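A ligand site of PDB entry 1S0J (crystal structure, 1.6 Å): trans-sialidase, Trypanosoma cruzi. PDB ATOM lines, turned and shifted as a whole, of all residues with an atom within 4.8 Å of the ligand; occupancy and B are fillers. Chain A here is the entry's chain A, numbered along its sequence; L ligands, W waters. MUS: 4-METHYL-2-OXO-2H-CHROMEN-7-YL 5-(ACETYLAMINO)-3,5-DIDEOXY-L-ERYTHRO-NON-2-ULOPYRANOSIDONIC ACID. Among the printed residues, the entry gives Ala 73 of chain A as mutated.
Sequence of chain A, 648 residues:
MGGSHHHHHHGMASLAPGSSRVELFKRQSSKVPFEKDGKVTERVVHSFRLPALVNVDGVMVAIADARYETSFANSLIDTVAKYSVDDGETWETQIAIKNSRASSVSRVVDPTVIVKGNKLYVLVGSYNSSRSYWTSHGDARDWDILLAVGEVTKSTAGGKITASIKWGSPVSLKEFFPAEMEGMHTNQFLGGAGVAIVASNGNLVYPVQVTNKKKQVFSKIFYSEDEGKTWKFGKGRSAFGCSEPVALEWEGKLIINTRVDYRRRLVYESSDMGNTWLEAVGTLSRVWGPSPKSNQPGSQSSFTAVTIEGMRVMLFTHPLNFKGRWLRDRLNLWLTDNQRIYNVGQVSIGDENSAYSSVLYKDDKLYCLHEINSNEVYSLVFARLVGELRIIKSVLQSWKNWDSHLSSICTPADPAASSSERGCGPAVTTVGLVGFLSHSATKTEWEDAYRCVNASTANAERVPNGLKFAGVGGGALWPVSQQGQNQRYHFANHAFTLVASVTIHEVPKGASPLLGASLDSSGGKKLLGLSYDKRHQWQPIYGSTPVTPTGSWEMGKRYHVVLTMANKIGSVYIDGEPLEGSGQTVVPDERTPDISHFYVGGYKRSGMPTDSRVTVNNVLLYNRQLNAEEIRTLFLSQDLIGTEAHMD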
ATOM      1  N   ARG A  49     -11.683   5.415   1.678  1.00  0.00           N
ATOM      2  CA  ARG A  49     -12.001   6.091   2.950  1.00  0.00           C
ATOM      3  C   ARG A  49     -13.426   6.609   2.889  1.00  0.00           C
ATOM      4  O   ARG A  49     -14.051   6.481   1.895  1.00  0.00           O
ATOM      5  CB  ARG A  49     -11.065   7.293   3.154  1.00  0.00           C
ATOM      6  CG  ARG A  49      -9.611   6.847   3.598  1.00  0.00           C
ATOM      7  CD  ARG A  49      -8.867   7.831   4.482  1.00  0.00           C
ATOM      8  NE  ARG A  49      -9.646   8.020   5.697  1.00  0.00           N
ATOM      9  CZ  ARG A  49      -9.462   8.997   6.569  1.00  0.00           C
ATOM     10  NH1 ARG A  49     -10.266   9.064   7.619  1.00  0.00           N
ATOM     11  NH2 ARG A  49      -8.503   9.905   6.375  1.00  0.00           N
ATOM     12  N   LEU A  50     -13.878   7.184   3.995  1.00  0.00           N
ATOM     13  CA  LEU A  50     -15.155   7.944   4.019  1.00  0.00           C
ATOM     14  C   LEU A  50     -16.372   7.063   3.744  1.00  0.00           C
ATOM     15  O   LEU A  50     -17.184   7.314   2.840  1.00  0.00           O
ATOM     16  CB  LEU A  50     -15.103   9.114   3.031  1.00  0.00           C
ATOM     17  CG  LEU A  50     -14.478  10.459   3.454  1.00  0.00           C
ATOM     18  CD1 LEU A  50     -15.545  11.255   4.239  1.00  0.00           C
ATOM     19  CD2 LEU A  50     -13.237  10.251   4.297  1.00  0.00           C
ATOM     20  N   ARG A  67      -9.323   6.638  -3.319  1.00  0.00           N
ATOM     21  CA  ARG A  67      -8.124   7.485  -3.403  1.00  0.00           C
ATOM     22  C   ARG A  67      -7.115   6.661  -4.195  1.00  0.00           C
ATOM     23  O   ARG A  67      -6.478   5.735  -3.666  1.00  0.00           O
ATOM     24  CB  ARG A  67      -7.609   7.850  -2.008  1.00  0.00           C
ATOM     25  CG  ARG A  67      -8.709   8.376  -1.067  1.00  0.00           C
ATOM     26  CD  ARG A  67      -8.202   9.251   0.009  1.00  0.00           C
ATOM     27  NE  ARG A  67      -9.332   9.820   0.797  1.00  0.00           N
ATOM     28  CZ  ARG A  67      -9.159  10.607   1.839  1.00  0.00           C
ATOM     29  NH1 ARG A  67      -7.929  10.892   2.269  1.00  0.00           N
ATOM     30  NH2 ARG A  67     -10.228  11.070   2.486  1.00  0.00           N
ATOM     31  N   ALA A  73      -5.264  13.359   1.646  1.00  0.00           N
ATOM     32  CA  ALA A  73      -6.555  13.967   1.343  1.00  0.00           C
ATOM     33  C   ALA A  73      -6.581  14.745   0.033  1.00  0.00           C
ATOM     34  O   ALA A  73      -7.613  14.827  -0.635  1.00  0.00           O
ATOM     35  CB  ALA A  73      -6.950  14.880   2.488  1.00  0.00           C
ATOM     36  N   ASN A  74      -5.467  15.391  -0.300  1.00  0.00           N
ATOM     37  CA  ASN A  74      -5.469  16.283  -1.456  1.00  0.00           C
ATOM     38  C   ASN A  74      -4.778  15.610  -2.615  1.00  0.00           C
ATOM     39  O   ASN A  74      -3.657  15.944  -3.021  1.00  0.00           O
ATOM     40  CB  ASN A  74      -4.810  17.600  -1.029  1.00  0.00           C
ATOM     41  CG  ASN A  74      -5.407  18.089   0.291  1.00  0.00           C
ATOM     42  OD1 ASN A  74      -6.624  18.143   0.436  1.00  0.00           O
ATOM     43  ND2 ASN A  74      -4.562  18.363   1.257  1.00  0.00           N
ATOM     44  N   VAL A 109     -14.796  15.047  -2.935  1.00  0.00           N
ATOM     45  CA  VAL A 109     -14.471  14.712  -1.577  1.00  0.00           C
ATOM     46  C   VAL A 109     -15.631  14.689  -0.594  1.00  0.00           C
ATOM     47  O   VAL A 109     -16.653  15.322  -0.777  1.00  0.00           O
ATOM     48  CB  VAL A 109     -13.389  15.645  -0.987  1.00  0.00           C
ATOM     49  CG1 VAL A 109     -12.039  15.517  -1.769  1.00  0.00           C
ATOM     50  CG2 VAL A 109     -13.905  17.083  -0.896  1.00  0.00           C
ATOM     51  N   ASP A 110     -15.390  13.944   0.472  1.00  0.00           N
ATOM     52  CA  ASP A 110     -16.295  13.793   1.622  1.00  0.00           C
ATOM     53  C   ASP A 110     -17.774  13.597   1.217  1.00  0.00           C
ATOM     54  O   ASP A 110     -18.663  14.343   1.634  1.00  0.00           O
ATOM     55  CB  ASP A 110     -16.074  14.952   2.609  1.00  0.00           C
ATOM     56  CG  ASP A 110     -14.635  14.959   3.191  1.00  0.00           C
ATOM     57  OD1 ASP A 110     -14.242  15.934   3.827  1.00  0.00           O
ATOM     58  OD2 ASP A 110     -13.851  14.004   3.033  1.00  0.00           O
ATOM     59  N   TYR A 133      -4.873  21.434   2.544  1.00  0.00           N
ATOM     60  CA  TYR A 133      -6.139  21.075   3.207  1.00  0.00           C
ATOM     61  C   TYR A 133      -7.145  22.207   3.050  1.00  0.00           C
ATOM     62  O   TYR A 133      -6.788  23.357   3.128  1.00  0.00           O
ATOM     63  CB  TYR A 133      -5.880  20.807   4.663  1.00  0.00           C
ATOM     64  CG  TYR A 133      -5.200  19.487   4.849  1.00  0.00           C
ATOM     65  CD1 TYR A 133      -3.863  19.406   5.169  1.00  0.00           C
ATOM     66  CD2 TYR A 133      -5.925  18.298   4.720  1.00  0.00           C
ATOM     67  CE1 TYR A 133      -3.257  18.166   5.374  1.00  0.00           C
ATOM     68  CE2 TYR A 133      -5.302  17.058   4.925  1.00  0.00           C
ATOM     69  CZ  TYR A 133      -3.965  17.025   5.228  1.00  0.00           C
ATOM     70  OH  TYR A 133      -3.313  15.807   5.436  1.00  0.00           O
ATOM     71  N   TRP A 134      -8.410  21.873   2.854  1.00  0.00           N
ATOM     72  CA  TRP A 134      -9.405  22.897   2.531  1.00  0.00           C
ATOM     73  C   TRP A 134      -9.542  24.023   3.532  1.00  0.00           C
ATOM     74  O   TRP A 134      -9.813  25.188   3.148  1.00  0.00           O
ATOM     75  CB  TRP A 134     -10.732  22.229   2.250  1.00  0.00           C
ATOM     76  CG  TRP A 134     -11.524  21.803   3.494  1.00  0.00           C
ATOM     77  CD1 TRP A 134     -11.243  20.790   4.353  1.00  0.00           C
ATOM     78  CD2 TRP A 134     -12.765  22.357   3.899  1.00  0.00           C
ATOM     79  NE1 TRP A 134     -12.247  20.685   5.311  1.00  0.00           N
ATOM     80  CE2 TRP A 134     -13.197  21.643   5.038  1.00  0.00           C
ATOM     81  CE3 TRP A 134     -13.554  23.409   3.424  1.00  0.00           C
ATOM     82  CZ2 TRP A 134     -14.371  21.945   5.710  1.00  0.00           C
ATOM     83  CZ3 TRP A 134     -14.716  23.716   4.076  1.00  0.00           C
ATOM     84  CH2 TRP A 134     -15.124  22.974   5.226  1.00  0.00           C
ATOM     85  N   THR A 135      -9.371  23.740   4.832  1.00  0.00           N
ATOM     86  CA  THR A 135      -9.560  24.807   5.812  1.00  0.00           C
ATOM     87  C   THR A 135      -8.382  25.793   5.838  1.00  0.00           C
ATOM     88  O   THR A 135      -8.439  26.853   6.454  1.00  0.00           O
ATOM     89  CB  THR A 135      -9.808  24.251   7.200  1.00  0.00           C
ATOM     90  OG1 THR A 135      -8.749  23.349   7.541  1.00  0.00           O
ATOM     91  CG2 THR A 135     -11.068  23.347   7.209  1.00  0.00           C
ATOM     92  N   LEU A 190     -18.651  21.935   2.674  1.00  0.00           N
ATOM     93  CA  LEU A 190     -18.720  20.495   2.394  1.00  0.00           C
ATOM     94  C   LEU A 190     -19.767  19.863   3.249  1.00  0.00           C
ATOM     95  O   LEU A 190     -20.154  20.382   4.292  1.00  0.00           O
ATOM     96  CB  LEU A 190     -17.379  19.813   2.743  1.00  0.00           C
ATOM     97  CG  LEU A 190     -16.130  20.380   2.097  1.00  0.00           C
ATOM     98  CD1 LEU A 190     -14.912  19.690   2.734  1.00  0.00           C
ATOM     99  CD2 LEU A 190     -16.173  20.135   0.568  1.00  0.00           C
ATOM    100  N   GLN A 209     -20.291  21.470   6.926  1.00  0.00           N
ATOM    101  CA  GLN A 209     -19.223  22.209   7.567  1.00  0.00           C
ATOM    102  C   GLN A 209     -18.813  23.330   6.598  1.00  0.00           C
ATOM    103  O   GLN A 209     -18.617  23.137   5.387  1.00  0.00           O
ATOM    104  CB  GLN A 209     -18.044  21.279   7.914  1.00  0.00           C
ATOM    105  CG  GLN A 209     -17.618  20.414   6.745  1.00  0.00           C
ATOM    106  CD  GLN A 209     -16.660  19.310   7.123  1.00  0.00           C
ATOM    107  OE1 GLN A 209     -15.843  19.444   8.048  1.00  0.00           O
ATOM    108  NE2 GLN A 209     -16.732  18.197   6.393  1.00  0.00           N
ATOM    109  N   SER A 243     -16.725  20.749  13.162  1.00  0.00           N
ATOM    110  CA  SER A 243     -16.675  20.299  11.783  1.00  0.00           C
ATOM    111  C   SER A 243     -17.349  18.933  11.660  1.00  0.00           C
ATOM    112  O   SER A 243     -17.897  18.418  12.653  1.00  0.00           O
ATOM    113  CB  SER A 243     -15.218  20.207  11.324  1.00  0.00           C
ATOM    114  OG  SER A 243     -14.631  19.087  11.964  1.00  0.00           O
ATOM    115  N   GLU A 244     -17.316  18.330  10.475  1.00  0.00           N
ATOM    116  CA  GLU A 244     -17.979  17.050  10.204  1.00  0.00           C
ATOM    117  C   GLU A 244     -19.216  16.806  11.030  1.00  0.00           C
ATOM    118  O   GLU A 244     -19.301  15.819  11.781  1.00  0.00           O
ATOM    119  CB  GLU A 244     -17.003  15.882  10.359  1.00  0.00           C
ATOM    120  CG  GLU A 244     -16.011  15.847   9.205  1.00  0.00           C
ATOM    121  CD  GLU A 244     -15.027  14.715   9.291  1.00  0.00           C
ATOM    122  OE1 GLU A 244     -14.902  14.137  10.383  1.00  0.00           O
ATOM    123  OE2 GLU A 244     -14.334  14.459   8.260  1.00  0.00           O
ATOM    124  N   ARG A 259     -17.928  17.109  15.328  1.00  0.00           N
ATOM    125  CA  ARG A 259     -16.501  16.904  15.540  1.00  0.00           C
ATOM    126  C   ARG A 259     -15.809  18.181  15.996  1.00  0.00           C
ATOM    127  O   ARG A 259     -15.993  19.225  15.395  1.00  0.00           O
ATOM    128  CB  ARG A 259     -15.859  16.362  14.268  1.00  0.00           C
ATOM    129  CG  ARG A 259     -14.252  16.199  14.403  1.00  0.00           C
ATOM    130  CD  ARG A 259     -13.759  15.653  13.086  1.00  0.00           C
ATOM    131  NE  ARG A 259     -12.307  15.692  13.029  1.00  0.00           N
ATOM    132  CZ  ARG A 259     -11.617  15.080  12.068  1.00  0.00           C
ATOM    133  NH1 ARG A 259     -12.216  14.365  11.172  1.00  0.00           N
ATOM    134  NH2 ARG A 259     -10.282  15.175  12.072  1.00  0.00           N
ATOM    135  N   TRP A 326      -4.039  11.120  14.402  1.00  0.00           N
ATOM    136  CA  TRP A 326      -5.182  10.740  13.573  1.00  0.00           C
ATOM    137  C   TRP A 326      -5.262   9.219  13.489  1.00  0.00           C
ATOM    138  O   TRP A 326      -6.085   8.676  12.750  1.00  0.00           O
ATOM    139  CB  TRP A 326      -5.084  11.351  12.160  1.00  0.00           C
ATOM    140  CG  TRP A 326      -5.353  12.868  12.115  1.00  0.00           C
ATOM    141  CD1 TRP A 326      -6.521  13.499  11.763  1.00  0.00           C
ATOM    142  CD2 TRP A 326      -4.425  13.915  12.411  1.00  0.00           C
ATOM    143  NE1 TRP A 326      -6.372  14.857  11.852  1.00  0.00           N
ATOM    144  CE2 TRP A 326      -5.095  15.138  12.251  1.00  0.00           C
ATOM    145  CE3 TRP A 326      -3.091  13.928  12.820  1.00  0.00           C
ATOM    146  CZ2 TRP A 326      -4.476  16.371  12.459  1.00  0.00           C
ATOM    147  CZ3 TRP A 326      -2.477  15.165  13.007  1.00  0.00           C
ATOM    148  CH2 TRP A 326      -3.182  16.360  12.849  1.00  0.00           C
ATOM    149  N   ARG A 328      -6.513   6.972  15.583  1.00  0.00           N
ATOM    150  CA  ARG A 328      -7.924   6.686  15.817  1.00  0.00           C
ATOM    151  C   ARG A 328      -8.307   5.213  15.847  1.00  0.00           C
ATOM    152  O   ARG A 328      -9.171   4.724  15.155  1.00  0.00           O
ATOM    153  CB  ARG A 328      -8.702   7.501  14.790  1.00  0.00           C
ATOM    154  CG  ARG A 328      -8.668   9.000  15.244  1.00  0.00           C
ATOM    155  CD  ARG A 328      -9.297   9.951  14.237  1.00  0.00           C
ATOM    156  NE  ARG A 328      -8.619   9.839  12.938  1.00  0.00           N
ATOM    157  CZ  ARG A 328      -8.906  10.593  11.890  1.00  0.00           C
ATOM    158  NH1 ARG A 328      -9.809  11.592  11.979  1.00  0.00           N
ATOM    159  NH2 ARG A 328      -8.273  10.382  10.738  1.00  0.00           N
ATOM    160  N   TYR A 356     -13.175   6.189  10.530  1.00  0.00           N
ATOM    161  CA  TYR A 356     -14.524   6.532  10.049  1.00  0.00           C
ATOM    162  C   TYR A 356     -15.393   5.314   9.911  1.00  0.00           C
ATOM    163  O   TYR A 356     -14.902   4.203   9.673  1.00  0.00           O
ATOM    164  CB  TYR A 356     -14.440   7.294   8.728  1.00  0.00           C
ATOM    165  CG  TYR A 356     -13.915   8.704   8.789  1.00  0.00           C
ATOM    166  CD1 TYR A 356     -13.077   9.161   9.816  1.00  0.00           C
ATOM    167  CD2 TYR A 356     -14.307   9.606   7.798  1.00  0.00           C
ATOM    168  CE1 TYR A 356     -12.632  10.511   9.840  1.00  0.00           C
ATOM    169  CE2 TYR A 356     -13.891  10.949   7.818  1.00  0.00           C
ATOM    170  CZ  TYR A 356     -13.047  11.382   8.818  1.00  0.00           C
ATOM    171  OH  TYR A 356     -12.686  12.719   8.779  1.00  0.00           O
ATOM    172  N   GLU A 376      -1.013   4.094   6.863  1.00  0.00           N
ATOM    173  CA  GLU A 376      -1.669   5.058   5.994  1.00  0.00           C
ATOM    174  C   GLU A 376      -2.134   4.464   4.659  1.00  0.00           C
ATOM    175  O   GLU A 376      -2.209   5.156   3.643  1.00  0.00           O
ATOM    176  CB  GLU A 376      -0.814   6.337   5.811  1.00  0.00           C
ATOM    177  CG  GLU A 376      -0.555   7.078   7.114  1.00  0.00           C
ATOM    178  CD  GLU A 376      -1.843   7.301   7.918  1.00  0.00           C
ATOM    179  OE1 GLU A 376      -2.837   7.874   7.335  1.00  0.00           O
ATOM    180  OE2 GLU A 376      -1.848   6.865   9.095  1.00  0.00           O
ATOM    181  N   TYR A 378      -5.580   2.528   3.511  1.00  0.00           N
ATOM    182  CA  TYR A 378      -6.863   2.237   4.142  1.00  0.00           C
ATOM    183  C   TYR A 378      -7.765   1.311   3.335  1.00  0.00           C
ATOM    184  O   TYR A 378      -7.898   1.458   2.107  1.00  0.00           O
ATOM    185  CB  TYR A 378      -7.663   3.558   4.265  1.00  0.00           C
ATOM    186  CG  TYR A 378      -7.034   4.647   5.131  1.00  0.00           C
ATOM    187  CD1 TYR A 378      -5.850   5.297   4.762  1.00  0.00           C
ATOM    188  CD2 TYR A 378      -7.645   5.040   6.336  1.00  0.00           C
ATOM    189  CE1 TYR A 378      -5.295   6.295   5.577  1.00  0.00           C
ATOM    190  CE2 TYR A 378      -7.101   6.052   7.133  1.00  0.00           C
ATOM    191  CZ  TYR A 378      -5.935   6.659   6.768  1.00  0.00           C
ATOM    192  OH  TYR A 378      -5.402   7.655   7.550  1.00  0.00           O
HETATM  193  O16 MUS L   1     -10.576  19.786   7.873  1.00  0.00           O
HETATM  194  C16 MUS L   1      -9.912  18.832   8.700  1.00  0.00           C
HETATM  195  C15 MUS L   1     -10.508  17.429   8.492  1.00  0.00           C
HETATM  196  O15 MUS L   1     -11.839  17.400   8.962  1.00  0.00           O
HETATM  197  C14 MUS L   1     -10.507  17.138   6.998  1.00  0.00           C
HETATM  198  O14 MUS L   1      -9.211  17.493   6.521  1.00  0.00           O
HETATM  199  C13 MUS L   1     -10.830  15.665   6.735  1.00  0.00           C
HETATM  200  O13 MUS L   1      -9.960  14.964   7.605  1.00  0.00           O
HETATM  201  C12 MUS L   1     -10.598  15.277   5.264  1.00  0.00           C
HETATM  202  N12 MUS L   1     -11.431  16.036   4.328  1.00  0.00           N
HETATM  203  C17 MUS L   1     -10.902  17.032   3.616  1.00  0.00           C
HETATM  204  C18 MUS L   1     -11.779  17.662   2.588  1.00  0.00           C
HETATM  205  O17 MUS L   1      -9.734  17.457   3.798  1.00  0.00           O
HETATM  206  C11 MUS L   1     -10.859  13.768   5.072  1.00  0.00           C
HETATM  207  O11 MUS L   1      -9.881  13.280   4.161  1.00  0.00           O
HETATM  208  C10 MUS L   1     -10.648  12.981   6.367  1.00  0.00           C
HETATM  209  C9  MUS L   1      -9.634  13.647   7.292  1.00  0.00           C
HETATM  210  C19 MUS L   1      -9.527  12.846   8.586  1.00  0.00           C
HETATM  211  O19 MUS L   1      -9.755  13.393   9.701  1.00  0.00           O
HETATM  212  O20 MUS L   1      -9.231  11.665   8.497  1.00  0.00           O
HETATM  213  O9  MUS L   1      -8.341  13.650   6.693  1.00  0.00           O
HETATM  214  C7  MUS L   1      -7.229  13.992   7.426  1.00  0.00           C
HETATM  215  C6  MUS L   1      -6.824  15.317   7.623  1.00  0.00           C
HETATM  216  C8  MUS L   1      -6.366  12.950   7.705  1.00  0.00           C
HETATM  217  C8A MUS L   1      -5.122  13.211   8.249  1.00  0.00           C
HETATM  218  C4A MUS L   1      -4.694  14.580   8.475  1.00  0.00           C
HETATM  219  C5  MUS L   1      -5.544  15.643   8.113  1.00  0.00           C
HETATM  220  O1  MUS L   1      -4.324  12.154   8.597  1.00  0.00           O
HETATM  221  C2  MUS L   1      -3.081  12.374   9.169  1.00  0.00           C
HETATM  222  O2  MUS L   1      -2.409  11.363   9.465  1.00  0.00           O
HETATM  223  C3  MUS L   1      -2.590  13.667   9.409  1.00  0.00           C
HETATM  224  C4  MUS L   1      -3.354  14.782   9.081  1.00  0.00           C
HETATM  225  CM4 MUS L   1      -2.886  16.160   9.328  1.00  0.00           C
HETATM  226  O   HOH W   1      -3.377   8.770  10.545  1.00  0.00           O
HETATM  227  O   HOH W   2      -8.691  19.118   1.872  1.00  0.00           O
HETATM  228  O   HOH W   3     -10.198  14.395   1.302  1.00  0.00           O
HETATM  229  O   HOH W   4     -11.803  20.985  10.067  1.00  0.00           O
HETATM  230  O   HOH W   5      -7.099  12.296   4.600  1.00  0.00           O
HETATM  231  O   HOH W   6     -13.353  18.635   7.399  1.00  0.00           O
HETATM  232  O   HOH W   7      -1.760  10.170  12.640  1.00  0.00           O
HETATM  233  O   HOH W   8     -11.881  18.623  11.519  1.00  0.00           O
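An oxygen (O19) of the ligand lies within salt-bridge range of the guanidinium group of Arg 259 (3.0 Å).
NE1 of Trp 134 lies within hydrogen-bond range of O16 of the ligand (3.2 Å).
The guanidinium group (NH2) of Arg 49 lies within salt-bridge range of an oxygen (O20) of the ligand (2.9 Å).
The guanidinium group (NH2) of Arg 328 is in salt-bridge range of an oxygen (O20) of the ligand, at 2.8 Å.
The guanidinium group of Arg 67 is in hydrogen-bond range of an oxygen (O11) of the ligand, at 2.8 Å.
A nitrogen (N12) of the ligand sits at hydrogen-bond distance from the side-chain carboxylate of Asp 110, 2.9 Å away.
An oxygen (O19) of the ligand is in hydrogen-bond range of the side-chain hydroxyl of Tyr 356 (3.1 Å).
The side-chain hydroxyl (OH) of Tyr 356 sits at hydrogen-bond distance from the guanidinium group (NH1) of Arg 259.
The backbone carbonyl oxygen of Trp 326 lies within hydrogen-bond range of the guanidinium group of Arg 328, 2.8 Å away.
N of Tyr 133 lies close to ND2 of Asn 74.
The side-chain hydroxyl (OH) of Tyr 356 is in hydrogen-bond range of the side-chain carboxylate (OE2) of Glu 244, at 2.5 Å.
The guanidinium group of Arg 259 lies within salt-bridge range of the side-chain carboxylate of Glu 244, 2.8 Å away.
O of Leu 190 lies within hydrogen-bond range of N of Gln 209 (2.9 Å).
The backbone carbonyl oxygen (O) of Arg 259 lies within hydrogen-bond range of the backbone NH (N) of Ser 243 (2.8 Å).
OE1 of Gln 209 sits at hydrogen-bond distance from N of Glu 244, 3.0 Å away.
CB of Ala 73 touches O11 of the ligand, at 3.7 Å.
Tyr 133 touches the ligand (OH to C5, 3.5 Å).
Thr 135 touches the ligand (CG2 to O16, 3.7 Å).
Leu 190 touches the ligand (CD1 to C18, 3.7 Å).
OE2 of Glu 244 touches O15 of the ligand (3.9 Å).
Trp 326 touches the ligand (CE3 to C3, 3.5 Å).
Hydrophobic or aromatic side chains that line the ligand: Ala 73, Tyr 133, Trp 134, Leu 190, Trp 326 and Tyr 356.
13 residues have an atom within 4 Å of the ligand: Arg 49, Arg 67, Ala 73, Asp 110, Tyr 133, Trp 134, Thr 135, Leu 190, Glu 244, Arg 259, Trp 326, Arg 328 and Tyr 356.
Water W6 lies within hydrogen-bond range of O15 of the ligand, OE1 of Gln 209 and NE1 of Trp 134.
Water W2 lies within hydrogen-bond range of OD1 of Asn 74, O17 of the ligand and N of Trp 134.
Water W5 lies within hydrogen-bond range of an oxygen (O9) of the ligand, the guanidinium group (NH1) of Arg 67 and the guanidinium group (NH2) of Arg 49.
Water W8 lies within hydrogen-bond range of OG of Ser 243 (2.8 Å), O15 of the ligand (2.8 Å) and NE of Arg 259 (3.3 Å).
Water W3 lies within hydrogen-bond range of an oxygen (O11) of the ligand and the backbone carbonyl oxygen of Ala 73.
Water W7 bridges the backbone NH (N) of Trp 326 (3.0 Å) and an oxygen (O2) of the ligand (3.5 Å).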
